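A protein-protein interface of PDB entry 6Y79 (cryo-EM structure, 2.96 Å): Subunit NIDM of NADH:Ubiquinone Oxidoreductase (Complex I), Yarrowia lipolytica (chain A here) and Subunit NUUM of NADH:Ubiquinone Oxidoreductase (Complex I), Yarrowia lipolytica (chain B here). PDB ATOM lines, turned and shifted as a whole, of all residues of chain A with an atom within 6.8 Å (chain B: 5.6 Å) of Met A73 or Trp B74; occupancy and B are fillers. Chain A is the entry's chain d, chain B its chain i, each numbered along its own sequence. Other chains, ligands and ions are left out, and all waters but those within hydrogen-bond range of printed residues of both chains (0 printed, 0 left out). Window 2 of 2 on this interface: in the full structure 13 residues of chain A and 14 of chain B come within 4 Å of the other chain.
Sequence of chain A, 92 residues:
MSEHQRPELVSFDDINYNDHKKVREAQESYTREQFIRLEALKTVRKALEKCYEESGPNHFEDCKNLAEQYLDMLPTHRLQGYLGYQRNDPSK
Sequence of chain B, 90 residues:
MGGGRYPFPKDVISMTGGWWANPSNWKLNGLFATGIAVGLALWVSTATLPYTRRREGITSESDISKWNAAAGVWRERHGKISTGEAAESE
Among the printed residues, merely in contact across the chains: Asn A65 with Ala B71 (3.6 Å), Leu A66 with Ala B71 (3.7 Å), Gln A69 with Ala B71 (3.3 Å), Gln A69 with Trp B74 (3.5 Å), Asp A72 with Lys B80 (3.5 Å) and Met A73 with Trp B74 (3.7 Å).
Hydrophobic or aromatic side chains of chain B that line the printed part of chain A: Ala B71 and Trp B74. Along chain B the printed residues that touch a printed residue of chain A span positions 71 to 80. Hydrophobic or aromatic side chains of chain A within 4 Å of the printed part of chain B: Leu A66 and Met A73.
The indole nitrogen (NE1) of Trp B74 lies within hydrogen-bond range of a ring nitrogen (NE2) of His B78 (3.2 Å). The backbone carbonyl oxygen (O) of Met A73 is in hydrogen-bond range of a ring nitrogen (ND1) of His A77 (2.8 Å). OG1 of Thr A76 lies within hydrogen-bond range of O of Met A73.
The side-chain carboxylate of Glu A68 is in salt-bridge range of the guanidinium group of Arg B75. NH2 of Arg B75 lies within hydrogen-bond range of OD1 of Asn A65 (2.6 Å).
Printed residues of chain B within 4 Å of Asp A72: Lys B80 (3.5 Å). Trp B74 touches two residues of chain A. Of the printed residues of chain A, Arg B75 touches Asn A65 (2.6 Å) and Glu A68 (3.4 Å). The nearest residue of chain A that does not touch Trp B74 is Asp A72 (4.4 Å). The nearest printed residue of chain B that does not touch Asp A72 is Trp B74 (4.4 Å).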
ATOM      1  N   ARG A  37      36.109   3.104 -24.756  1.00  0.00           N
ATOM      2  CA  ARG A  37      34.796   3.748 -24.670  1.00  0.00           C
ATOM      3  C   ARG A  37      34.896   5.271 -24.644  1.00  0.00           C
ATOM      4  O   ARG A  37      34.141   5.988 -25.331  1.00  0.00           O
ATOM      5  CB  ARG A  37      34.127   3.244 -23.398  1.00  0.00           C
ATOM      6  CG  ARG A  37      32.677   3.437 -23.311  1.00  0.00           C
ATOM      7  CD  ARG A  37      32.109   2.643 -22.172  1.00  0.00           C
ATOM      8  NE  ARG A  37      30.668   2.516 -22.320  1.00  0.00           N
ATOM      9  CZ  ARG A  37      29.848   2.145 -21.349  1.00  0.00           C
ATOM     10  NH1 ARG A  37      28.548   2.051 -21.574  1.00  0.00           N
ATOM     11  NH2 ARG A  37      30.331   1.893 -20.146  1.00  0.00           N
ATOM     12  N   ALA A  40      35.906   6.826 -27.954  1.00  0.00           N
ATOM     13  CA  ALA A  40      34.728   6.861 -28.823  1.00  0.00           C
ATOM     14  C   ALA A  40      33.874   8.102 -28.557  1.00  0.00           C
ATOM     15  O   ALA A  40      33.437   8.789 -29.501  1.00  0.00           O
ATOM     16  CB  ALA A  40      33.903   5.592 -28.639  1.00  0.00           C
ATOM     17  N   LEU A  41      33.663   8.424 -27.274  1.00  0.00           N
ATOM     18  CA  LEU A  41      32.919   9.638 -26.912  1.00  0.00           C
ATOM     19  C   LEU A  41      33.622  10.910 -27.399  1.00  0.00           C
ATOM     20  O   LEU A  41      32.979  11.841 -27.910  1.00  0.00           O
ATOM     21  CB  LEU A  41      32.720   9.688 -25.400  1.00  0.00           C
ATOM     22  CG  LEU A  41      32.227  11.001 -24.802  1.00  0.00           C
ATOM     23  CD1 LEU A  41      30.789  11.237 -25.183  1.00  0.00           C
ATOM     24  CD2 LEU A  41      32.385  11.011 -23.305  1.00  0.00           C
ATOM     25  N   LYS A  42      34.952  10.955 -27.273  1.00  0.00           N
ATOM     26  CA  LYS A  42      35.706  12.124 -27.727  1.00  0.00           C
ATOM     27  C   LYS A  42      35.690  12.272 -29.245  1.00  0.00           C
ATOM     28  O   LYS A  42      35.688  13.402 -29.756  1.00  0.00           O
ATOM     29  CB  LYS A  42      37.146  12.045 -27.246  1.00  0.00           C
ATOM     30  CG  LYS A  42      37.310  12.187 -25.759  1.00  0.00           C
ATOM     31  CD  LYS A  42      38.770  12.137 -25.397  1.00  0.00           C
ATOM     32  CE  LYS A  42      38.957  12.243 -23.911  1.00  0.00           C
ATOM     33  NZ  LYS A  42      40.393  12.244 -23.561  1.00  0.00           N
ATOM     34  N   VAL A  44      33.163  11.426 -31.179  1.00  0.00           N
ATOM     35  CA  VAL A  44      31.876  12.028 -31.526  1.00  0.00           C
ATOM     36  C   VAL A  44      31.827  13.509 -31.149  1.00  0.00           C
ATOM     37  O   VAL A  44      31.226  14.314 -31.871  1.00  0.00           O
ATOM     38  CB  VAL A  44      30.732  11.232 -30.884  1.00  0.00           C
ATOM     39  CG1 VAL A  44      29.373  11.789 -31.275  1.00  0.00           C
ATOM     40  CG2 VAL A  44      30.824   9.790 -31.301  1.00  0.00           C
ATOM     41  N   ARG A  45      32.497  13.908 -30.060  1.00  0.00           N
ATOM     42  CA  ARG A  45      32.538  15.328 -29.695  1.00  0.00           C
ATOM     43  C   ARG A  45      33.276  16.172 -30.734  1.00  0.00           C
ATOM     44  O   ARG A  45      32.810  17.258 -31.106  1.00  0.00           O
ATOM     45  CB  ARG A  45      33.192  15.504 -28.329  1.00  0.00           C
ATOM     46  CG  ARG A  45      33.100  16.908 -27.784  1.00  0.00           C
ATOM     47  CD  ARG A  45      33.645  17.001 -26.376  1.00  0.00           C
ATOM     48  NE  ARG A  45      35.077  16.747 -26.318  1.00  0.00           N
ATOM     49  CZ  ARG A  45      35.650  15.893 -25.479  1.00  0.00           C
ATOM     50  NH1 ARG A  45      36.964  15.724 -25.500  1.00  0.00           N
ATOM     51  NH2 ARG A  45      34.912  15.218 -24.615  1.00  0.00           N
ATOM     52  N   ASN A  65      21.124  15.034 -34.649  1.00  0.00           N
ATOM     53  CA  ASN A  65      21.397  13.666 -34.213  1.00  0.00           C
ATOM     54  C   ASN A  65      22.788  13.523 -33.603  1.00  0.00           C
ATOM     55  O   ASN A  65      22.968  12.741 -32.667  1.00  0.00           O
ATOM     56  CB  ASN A  65      21.224  12.682 -35.369  1.00  0.00           C
ATOM     57  CG  ASN A  65      19.775  12.497 -35.770  1.00  0.00           C
ATOM     58  OD1 ASN A  65      18.897  12.370 -34.920  1.00  0.00           O
ATOM     59  ND2 ASN A  65      19.521  12.469 -37.072  1.00  0.00           N
ATOM     60  N   LEU A  66      23.776  14.284 -34.086  1.00  0.00           N
ATOM     61  CA  LEU A  66      25.097  14.259 -33.456  1.00  0.00           C
ATOM     62  C   LEU A  66      25.061  14.867 -32.059  1.00  0.00           C
ATOM     63  O   LEU A  66      25.722  14.369 -31.140  1.00  0.00           O
ATOM     64  CB  LEU A  66      26.118  14.999 -34.313  1.00  0.00           C
ATOM     65  CG  LEU A  66      26.733  14.288 -35.509  1.00  0.00           C
ATOM     66  CD1 LEU A  66      27.660  15.228 -36.250  1.00  0.00           C
ATOM     67  CD2 LEU A  66      27.484  13.065 -35.051  1.00  0.00           C
ATOM     68  N   GLU A  68      22.335  15.033 -30.046  1.00  0.00           N
ATOM     69  CA  GLU A  68      21.626  14.054 -29.230  1.00  0.00           C
ATOM     70  C   GLU A  68      22.501  12.857 -28.903  1.00  0.00           C
ATOM     71  O   GLU A  68      22.424  12.330 -27.792  1.00  0.00           O
ATOM     72  CB  GLU A  68      20.359  13.573 -29.936  1.00  0.00           C
ATOM     73  CG  GLU A  68      19.308  14.629 -30.186  1.00  0.00           C
ATOM     74  CD  GLU A  68      18.325  14.770 -29.061  1.00  0.00           C
ATOM     75  OE1 GLU A  68      17.856  13.744 -28.540  1.00  0.00           O
ATOM     76  OE2 GLU A  68      18.009  15.912 -28.696  1.00  0.00           O
ATOM     77  N   GLN A  69      23.351  12.432 -29.840  1.00  0.00           N
ATOM     78  CA  GLN A  69      24.232  11.302 -29.589  1.00  0.00           C
ATOM     79  C   GLN A  69      25.274  11.638 -28.532  1.00  0.00           C
ATOM     80  O   GLN A  69      25.534  10.830 -27.633  1.00  0.00           O
ATOM     81  CB  GLN A  69      24.909  10.874 -30.884  1.00  0.00           C
ATOM     82  CG  GLN A  69      25.952   9.815 -30.676  1.00  0.00           C
ATOM     83  CD  GLN A  69      26.692   9.486 -31.926  1.00  0.00           C
ATOM     84  OE1 GLN A  69      26.643  10.234 -32.894  1.00  0.00           O
ATOM     85  NE2 GLN A  69      27.403   8.371 -31.915  1.00  0.00           N
ATOM     86  N   TYR A  70      25.875  12.831 -28.623  1.00  0.00           N
ATOM     87  CA  TYR A  70      26.848  13.254 -27.619  1.00  0.00           C
ATOM     88  C   TYR A  70      26.205  13.379 -26.247  1.00  0.00           C
ATOM     89  O   TYR A  70      26.768  12.934 -25.244  1.00  0.00           O
ATOM     90  CB  TYR A  70      27.504  14.577 -28.008  1.00  0.00           C
ATOM     91  CG  TYR A  70      28.493  15.062 -26.968  1.00  0.00           C
ATOM     92  CD1 TYR A  70      29.738  14.472 -26.851  1.00  0.00           C
ATOM     93  CD2 TYR A  70      28.174  16.095 -26.092  1.00  0.00           C
ATOM     94  CE1 TYR A  70      30.637  14.894 -25.900  1.00  0.00           C
ATOM     95  CE2 TYR A  70      29.070  16.521 -25.136  1.00  0.00           C
ATOM     96  CZ  TYR A  70      30.301  15.919 -25.050  1.00  0.00           C
ATOM     97  OH  TYR A  70      31.205  16.339 -24.107  1.00  0.00           O
ATOM     98  N   LEU A  71      25.017  13.969 -26.178  1.00  0.00           N
ATOM     99  CA  LEU A  71      24.428  14.157 -24.862  1.00  0.00           C
ATOM    100  C   LEU A  71      23.754  12.896 -24.335  1.00  0.00           C
ATOM    101  O   LEU A  71      23.394  12.854 -23.155  1.00  0.00           O
ATOM    102  CB  LEU A  71      23.442  15.314 -24.895  1.00  0.00           C
ATOM    103  CG  LEU A  71      23.971  16.721 -25.128  1.00  0.00           C
ATOM    104  CD1 LEU A  71      22.787  17.637 -25.335  1.00  0.00           C
ATOM    105  CD2 LEU A  71      24.830  17.180 -23.961  1.00  0.00           C
ATOM    106  N   ASP A  72      23.562  11.875 -25.172  1.00  0.00           N
ATOM    107  CA  ASP A  72      23.118  10.582 -24.664  1.00  0.00           C
ATOM    108  C   ASP A  72      24.287   9.720 -24.215  1.00  0.00           C
ATOM    109  O   ASP A  72      24.149   8.937 -23.273  1.00  0.00           O
ATOM    110  CB  ASP A  72      22.315   9.830 -25.726  1.00  0.00           C
ATOM    111  CG  ASP A  72      20.922  10.386 -25.912  1.00  0.00           C
ATOM    112  OD1 ASP A  72      20.369  10.954 -24.950  1.00  0.00           O
ATOM    113  OD2 ASP A  72      20.380  10.254 -27.028  1.00  0.00           O
ATOM    114  N   MET A  73      25.436   9.845 -24.881  1.00  0.00           N
ATOM    115  CA  MET A  73      26.603   9.057 -24.508  1.00  0.00           C
ATOM    116  C   MET A  73      27.258   9.564 -23.236  1.00  0.00           C
ATOM    117  O   MET A  73      27.937   8.796 -22.549  1.00  0.00           O
ATOM    118  CB  MET A  73      27.635   9.087 -25.622  1.00  0.00           C
ATOM    119  CG  MET A  73      27.469   8.050 -26.688  1.00  0.00           C
ATOM    120  SD  MET A  73      28.795   8.219 -27.874  1.00  0.00           S
ATOM    121  CE  MET A  73      28.756   9.990 -28.085  1.00  0.00           C
ATOM    122  N   LEU A  74      27.101  10.850 -22.935  1.00  0.00           N
ATOM    123  CA  LEU A  74      27.863  11.473 -21.853  1.00  0.00           C
ATOM    124  C   LEU A  74      27.580  10.936 -20.444  1.00  0.00           C
ATOM    125  O   LEU A  74      28.553  10.795 -19.683  1.00  0.00           O
ATOM    126  CB  LEU A  74      27.666  12.994 -21.916  1.00  0.00           C
ATOM    127  CG  LEU A  74      28.441  13.869 -20.938  1.00  0.00           C
ATOM    128  CD1 LEU A  74      29.927  13.794 -21.201  1.00  0.00           C
ATOM    129  CD2 LEU A  74      27.952  15.274 -21.061  1.00  0.00           C
ATOM    130  N   PRO A  75      26.344  10.614 -20.019  1.00  0.00           N
ATOM    131  CA  PRO A  75      26.203  10.017 -18.680  1.00  0.00           C
ATOM    132  C   PRO A  75      26.717   8.595 -18.566  1.00  0.00           C
ATOM    133  O   PRO A  75      26.879   8.109 -17.441  1.00  0.00           O
ATOM    134  CB  PRO A  75      24.693  10.068 -18.427  1.00  0.00           C
ATOM    135  CG  PRO A  75      24.217  11.137 -19.272  1.00  0.00           C
ATOM    136  CD  PRO A  75      25.012  11.012 -20.514  1.00  0.00           C
ATOM    137  N   THR A  76      26.979   7.904 -19.675  1.00  0.00           N
ATOM    138  CA  THR A  76      27.299   6.488 -19.628  1.00  0.00           C
ATOM    139  C   THR A  76      28.701   6.146 -20.108  1.00  0.00           C
ATOM    140  O   THR A  76      29.132   5.007 -19.916  1.00  0.00           O
ATOM    141  CB  THR A  76      26.286   5.687 -20.458  1.00  0.00           C
ATOM    142  OG1 THR A  76      26.370   6.087 -21.828  1.00  0.00           O
ATOM    143  CG2 THR A  76      24.867   5.926 -19.958  1.00  0.00           C
ATOM    144  N   HIS A  77      29.423   7.079 -20.718  1.00  0.00           N
ATOM    145  CA  HIS A  77      30.738   6.796 -21.291  1.00  0.00           C
ATOM    146  C   HIS A  77      31.781   7.588 -20.516  1.00  0.00           C
ATOM    147  O   HIS A  77      32.174   8.683 -20.917  1.00  0.00           O
ATOM    148  CB  HIS A  77      30.779   7.132 -22.772  1.00  0.00           C
ATOM    149  CG  HIS A  77      29.906   6.262 -23.617  1.00  0.00           C
ATOM    150  ND1 HIS A  77      28.537   6.216 -23.472  1.00  0.00           N
ATOM    151  CD2 HIS A  77      30.200   5.429 -24.640  1.00  0.00           C
ATOM    152  CE1 HIS A  77      28.030   5.374 -24.353  1.00  0.00           C
ATOM    153  NE2 HIS A  77      29.020   4.881 -25.073  1.00  0.00           N
ATOM    154  N   ARG A  78      32.248   7.017 -19.415  1.00  0.00           N
ATOM    155  CA  ARG A  78      33.274   7.632 -18.593  1.00  0.00           C
ATOM    156  C   ARG A  78      33.997   6.531 -17.835  1.00  0.00           C
ATOM    157  O   ARG A  78      33.705   5.344 -17.998  1.00  0.00           O
ATOM    158  CB  ARG A  78      32.669   8.657 -17.639  1.00  0.00           C
ATOM    159  CG  ARG A  78      31.672   8.056 -16.688  1.00  0.00           C
ATOM    160  CD  ARG A  78      31.022   9.131 -15.864  1.00  0.00           C
ATOM    161  NE  ARG A  78      30.208  10.011 -16.687  1.00  0.00           N
ATOM    162  CZ  ARG A  78      29.685  11.151 -16.259  1.00  0.00           C
ATOM    163  NH1 ARG A  78      29.894  11.547 -15.014  1.00  0.00           N
ATOM    164  NH2 ARG A  78      28.953  11.892 -17.074  1.00  0.00           N
ATOM    165  N   ALA B  69      24.041  10.870 -40.529  1.00  0.00           N
ATOM    166  CA  ALA B  69      23.441   9.579 -40.861  1.00  0.00           C
ATOM    167  C   ALA B  69      23.881   8.490 -39.880  1.00  0.00           C
ATOM    168  O   ALA B  69      23.057   7.703 -39.399  1.00  0.00           O
ATOM    169  CB  ALA B  69      23.804   9.196 -42.297  1.00  0.00           C
ATOM    170  N   ALA B  70      25.173   8.449 -39.548  1.00  0.00           N
ATOM    171  CA  ALA B  70      25.675   7.456 -38.598  1.00  0.00           C
ATOM    172  C   ALA B  70      25.216   7.735 -37.176  1.00  0.00           C
ATOM    173  O   ALA B  70      25.119   6.811 -36.364  1.00  0.00           O
ATOM    174  CB  ALA B  70      27.195   7.397 -38.641  1.00  0.00           C
ATOM    175  N   ALA B  71      24.946   8.994 -36.845  1.00  0.00           N
ATOM    176  CA  ALA B  71      24.339   9.290 -35.556  1.00  0.00           C
ATOM    177  C   ALA B  71      22.899   8.805 -35.518  1.00  0.00           C
ATOM    178  O   ALA B  71      22.429   8.323 -34.485  1.00  0.00           O
ATOM    179  CB  ALA B  71      24.416  10.786 -35.265  1.00  0.00           C
ATOM    180  N   GLY B  72      22.188   8.908 -36.641  1.00  0.00           N
ATOM    181  CA  GLY B  72      20.888   8.265 -36.743  1.00  0.00           C
ATOM    182  C   GLY B  72      20.942   6.755 -36.663  1.00  0.00           C
ATOM    183  O   GLY B  72      20.012   6.120 -36.162  1.00  0.00           O
ATOM    184  N   VAL B  73      22.040   6.170 -37.139  1.00  0.00           N
ATOM    185  CA  VAL B  73      22.248   4.722 -37.036  1.00  0.00           C
ATOM    186  C   VAL B  73      22.431   4.352 -35.559  1.00  0.00           C
ATOM    187  O   VAL B  73      21.874   3.371 -35.008  1.00  0.00           O
ATOM    188  CB  VAL B  73      23.467   4.313 -37.880  1.00  0.00           C
ATOM    189  CG1 VAL B  73      23.969   2.953 -37.511  1.00  0.00           C
ATOM    190  CG2 VAL B  73      23.088   4.407 -39.349  1.00  0.00           C
ATOM    191  N   TRP B  74      23.285   5.130 -34.871  1.00  0.00           N
ATOM    192  CA  TRP B  74      23.560   4.823 -33.441  1.00  0.00           C
ATOM    193  C   TRP B  74      22.340   5.113 -32.590  1.00  0.00           C
ATOM    194  O   TRP B  74      22.116   4.430 -31.607  1.00  0.00           O
ATOM    195  CB  TRP B  74      24.813   5.522 -33.028  1.00  0.00           C
ATOM    196  CG  TRP B  74      25.201   5.156 -31.690  1.00  0.00           C
ATOM    197  CD1 TRP B  74      25.943   4.088 -31.300  1.00  0.00           C
ATOM    198  CD2 TRP B  74      24.766   5.801 -30.512  1.00  0.00           C
ATOM    199  NE1 TRP B  74      26.024   4.053 -29.938  1.00  0.00           N
ATOM    200  CE2 TRP B  74      25.300   5.100 -29.431  1.00  0.00           C
ATOM    201  CE3 TRP B  74      23.974   6.921 -30.271  1.00  0.00           C
ATOM    202  CZ2 TRP B  74      25.077   5.486 -28.122  1.00  0.00           C
ATOM    203  CZ3 TRP B  74      23.755   7.308 -28.984  1.00  0.00           C
ATOM    204  CH2 TRP B  74      24.300   6.593 -27.916  1.00  0.00           C
ATOM    205  N   ARG B  75      21.494   6.062 -33.020  1.00  0.00           N
ATOM    206  CA  ARG B  75      20.217   6.268 -32.355  1.00  0.00           C
ATOM    207  C   ARG B  75      19.154   5.239 -32.758  1.00  0.00           C
ATOM    208  O   ARG B  75      18.209   5.058 -31.983  1.00  0.00           O
ATOM    209  CB  ARG B  75      19.761   7.731 -32.605  1.00  0.00           C
ATOM    210  CG  ARG B  75      18.821   8.346 -31.588  1.00  0.00           C
ATOM    211  CD  ARG B  75      18.783   9.869 -31.775  1.00  0.00           C
ATOM    212  NE  ARG B  75      17.491  10.459 -31.444  1.00  0.00           N
ATOM    213  CZ  ARG B  75      17.129  11.691 -31.788  1.00  0.00           C
ATOM    214  NH1 ARG B  75      15.931  12.153 -31.453  1.00  0.00           N
ATOM    215  NH2 ARG B  75      17.958  12.457 -32.480  1.00  0.00           N
ATOM    216  N   GLU B  76      19.237   4.576 -33.937  1.00  0.00           N
ATOM    217  CA  GLU B  76      18.210   3.558 -34.183  1.00  0.00           C
ATOM    218  C   GLU B  76      18.467   2.359 -33.302  1.00  0.00           C
ATOM    219  O   GLU B  76      17.537   1.759 -32.766  1.00  0.00           O
ATOM    220  CB  GLU B  76      18.056   3.081 -35.645  1.00  0.00           C
ATOM    221  CG  GLU B  76      19.290   2.513 -36.471  1.00  0.00           C
ATOM    222  CD  GLU B  76      19.763   1.053 -36.165  1.00  0.00           C
ATOM    223  OE1 GLU B  76      18.983   0.151 -35.748  1.00  0.00           O
ATOM    224  OE2 GLU B  76      20.974   0.857 -36.299  1.00  0.00           O
ATOM    225  N   ARG B  77      19.721   1.973 -33.152  1.00  0.00           N
ATOM    226  CA  ARG B  77      19.955   0.687 -32.494  1.00  0.00           C
ATOM    227  C   ARG B  77      19.662   0.707 -30.979  1.00  0.00           C
ATOM    228  O   ARG B  77      19.305  -0.335 -30.428  1.00  0.00           O
ATOM    229  CB  ARG B  77      21.370   0.192 -32.822  1.00  0.00           C
ATOM    230  CG  ARG B  77      22.377   1.020 -32.174  1.00  0.00           C
ATOM    231  CD  ARG B  77      23.728   0.453 -32.369  1.00  0.00           C
ATOM    232  NE  ARG B  77      24.020   0.345 -33.786  1.00  0.00           N
ATOM    233  CZ  ARG B  77      25.043  -0.337 -34.272  1.00  0.00           C
ATOM    234  NH1 ARG B  77      25.241  -0.392 -35.580  1.00  0.00           N
ATOM    235  NH2 ARG B  77      25.862  -0.970 -33.448  1.00  0.00           N
ATOM    236  N   HIS B  78      19.673   1.862 -30.316  1.00  0.00           N
ATOM    237  CA  HIS B  78      19.387   1.945 -28.886  1.00  0.00           C
ATOM    238  C   HIS B  78      17.947   2.337 -28.579  1.00  0.00           C
ATOM    239  O   HIS B  78      17.577   2.402 -27.401  1.00  0.00           O
ATOM    240  CB  HIS B  78      20.368   2.918 -28.226  1.00  0.00           C
ATOM    241  CG  HIS B  78      21.783   2.441 -28.281  1.00  0.00           C
ATOM    242  ND1 HIS B  78      22.278   1.475 -27.436  1.00  0.00           N
ATOM    243  CD2 HIS B  78      22.791   2.751 -29.125  1.00  0.00           C
ATOM    244  CE1 HIS B  78      23.540   1.232 -27.740  1.00  0.00           C
ATOM    245  NE2 HIS B  78      23.875   1.995 -28.762  1.00  0.00           N
ATOM    246  N   LYS B  80      16.495   5.080 -28.901  1.00  0.00           N
ATOM    247  CA  LYS B  80      16.468   6.331 -28.163  1.00  0.00           C
ATOM    248  C   LYS B  80      15.562   7.321 -28.857  1.00  0.00           C
ATOM    249  O   LYS B  80      15.721   7.619 -30.040  1.00  0.00           O
ATOM    250  CB  LYS B  80      17.860   6.909 -27.988  1.00  0.00           C
ATOM    251  CG  LYS B  80      18.663   6.119 -27.031  1.00  0.00           C
ATOM    252  CD  LYS B  80      20.001   6.739 -26.880  1.00  0.00           C
ATOM    253  CE  LYS B  80      20.897   5.841 -26.072  1.00  0.00           C
ATOM    254  NZ  LYS B  80      20.403   5.647 -24.689  1.00  0.00           N
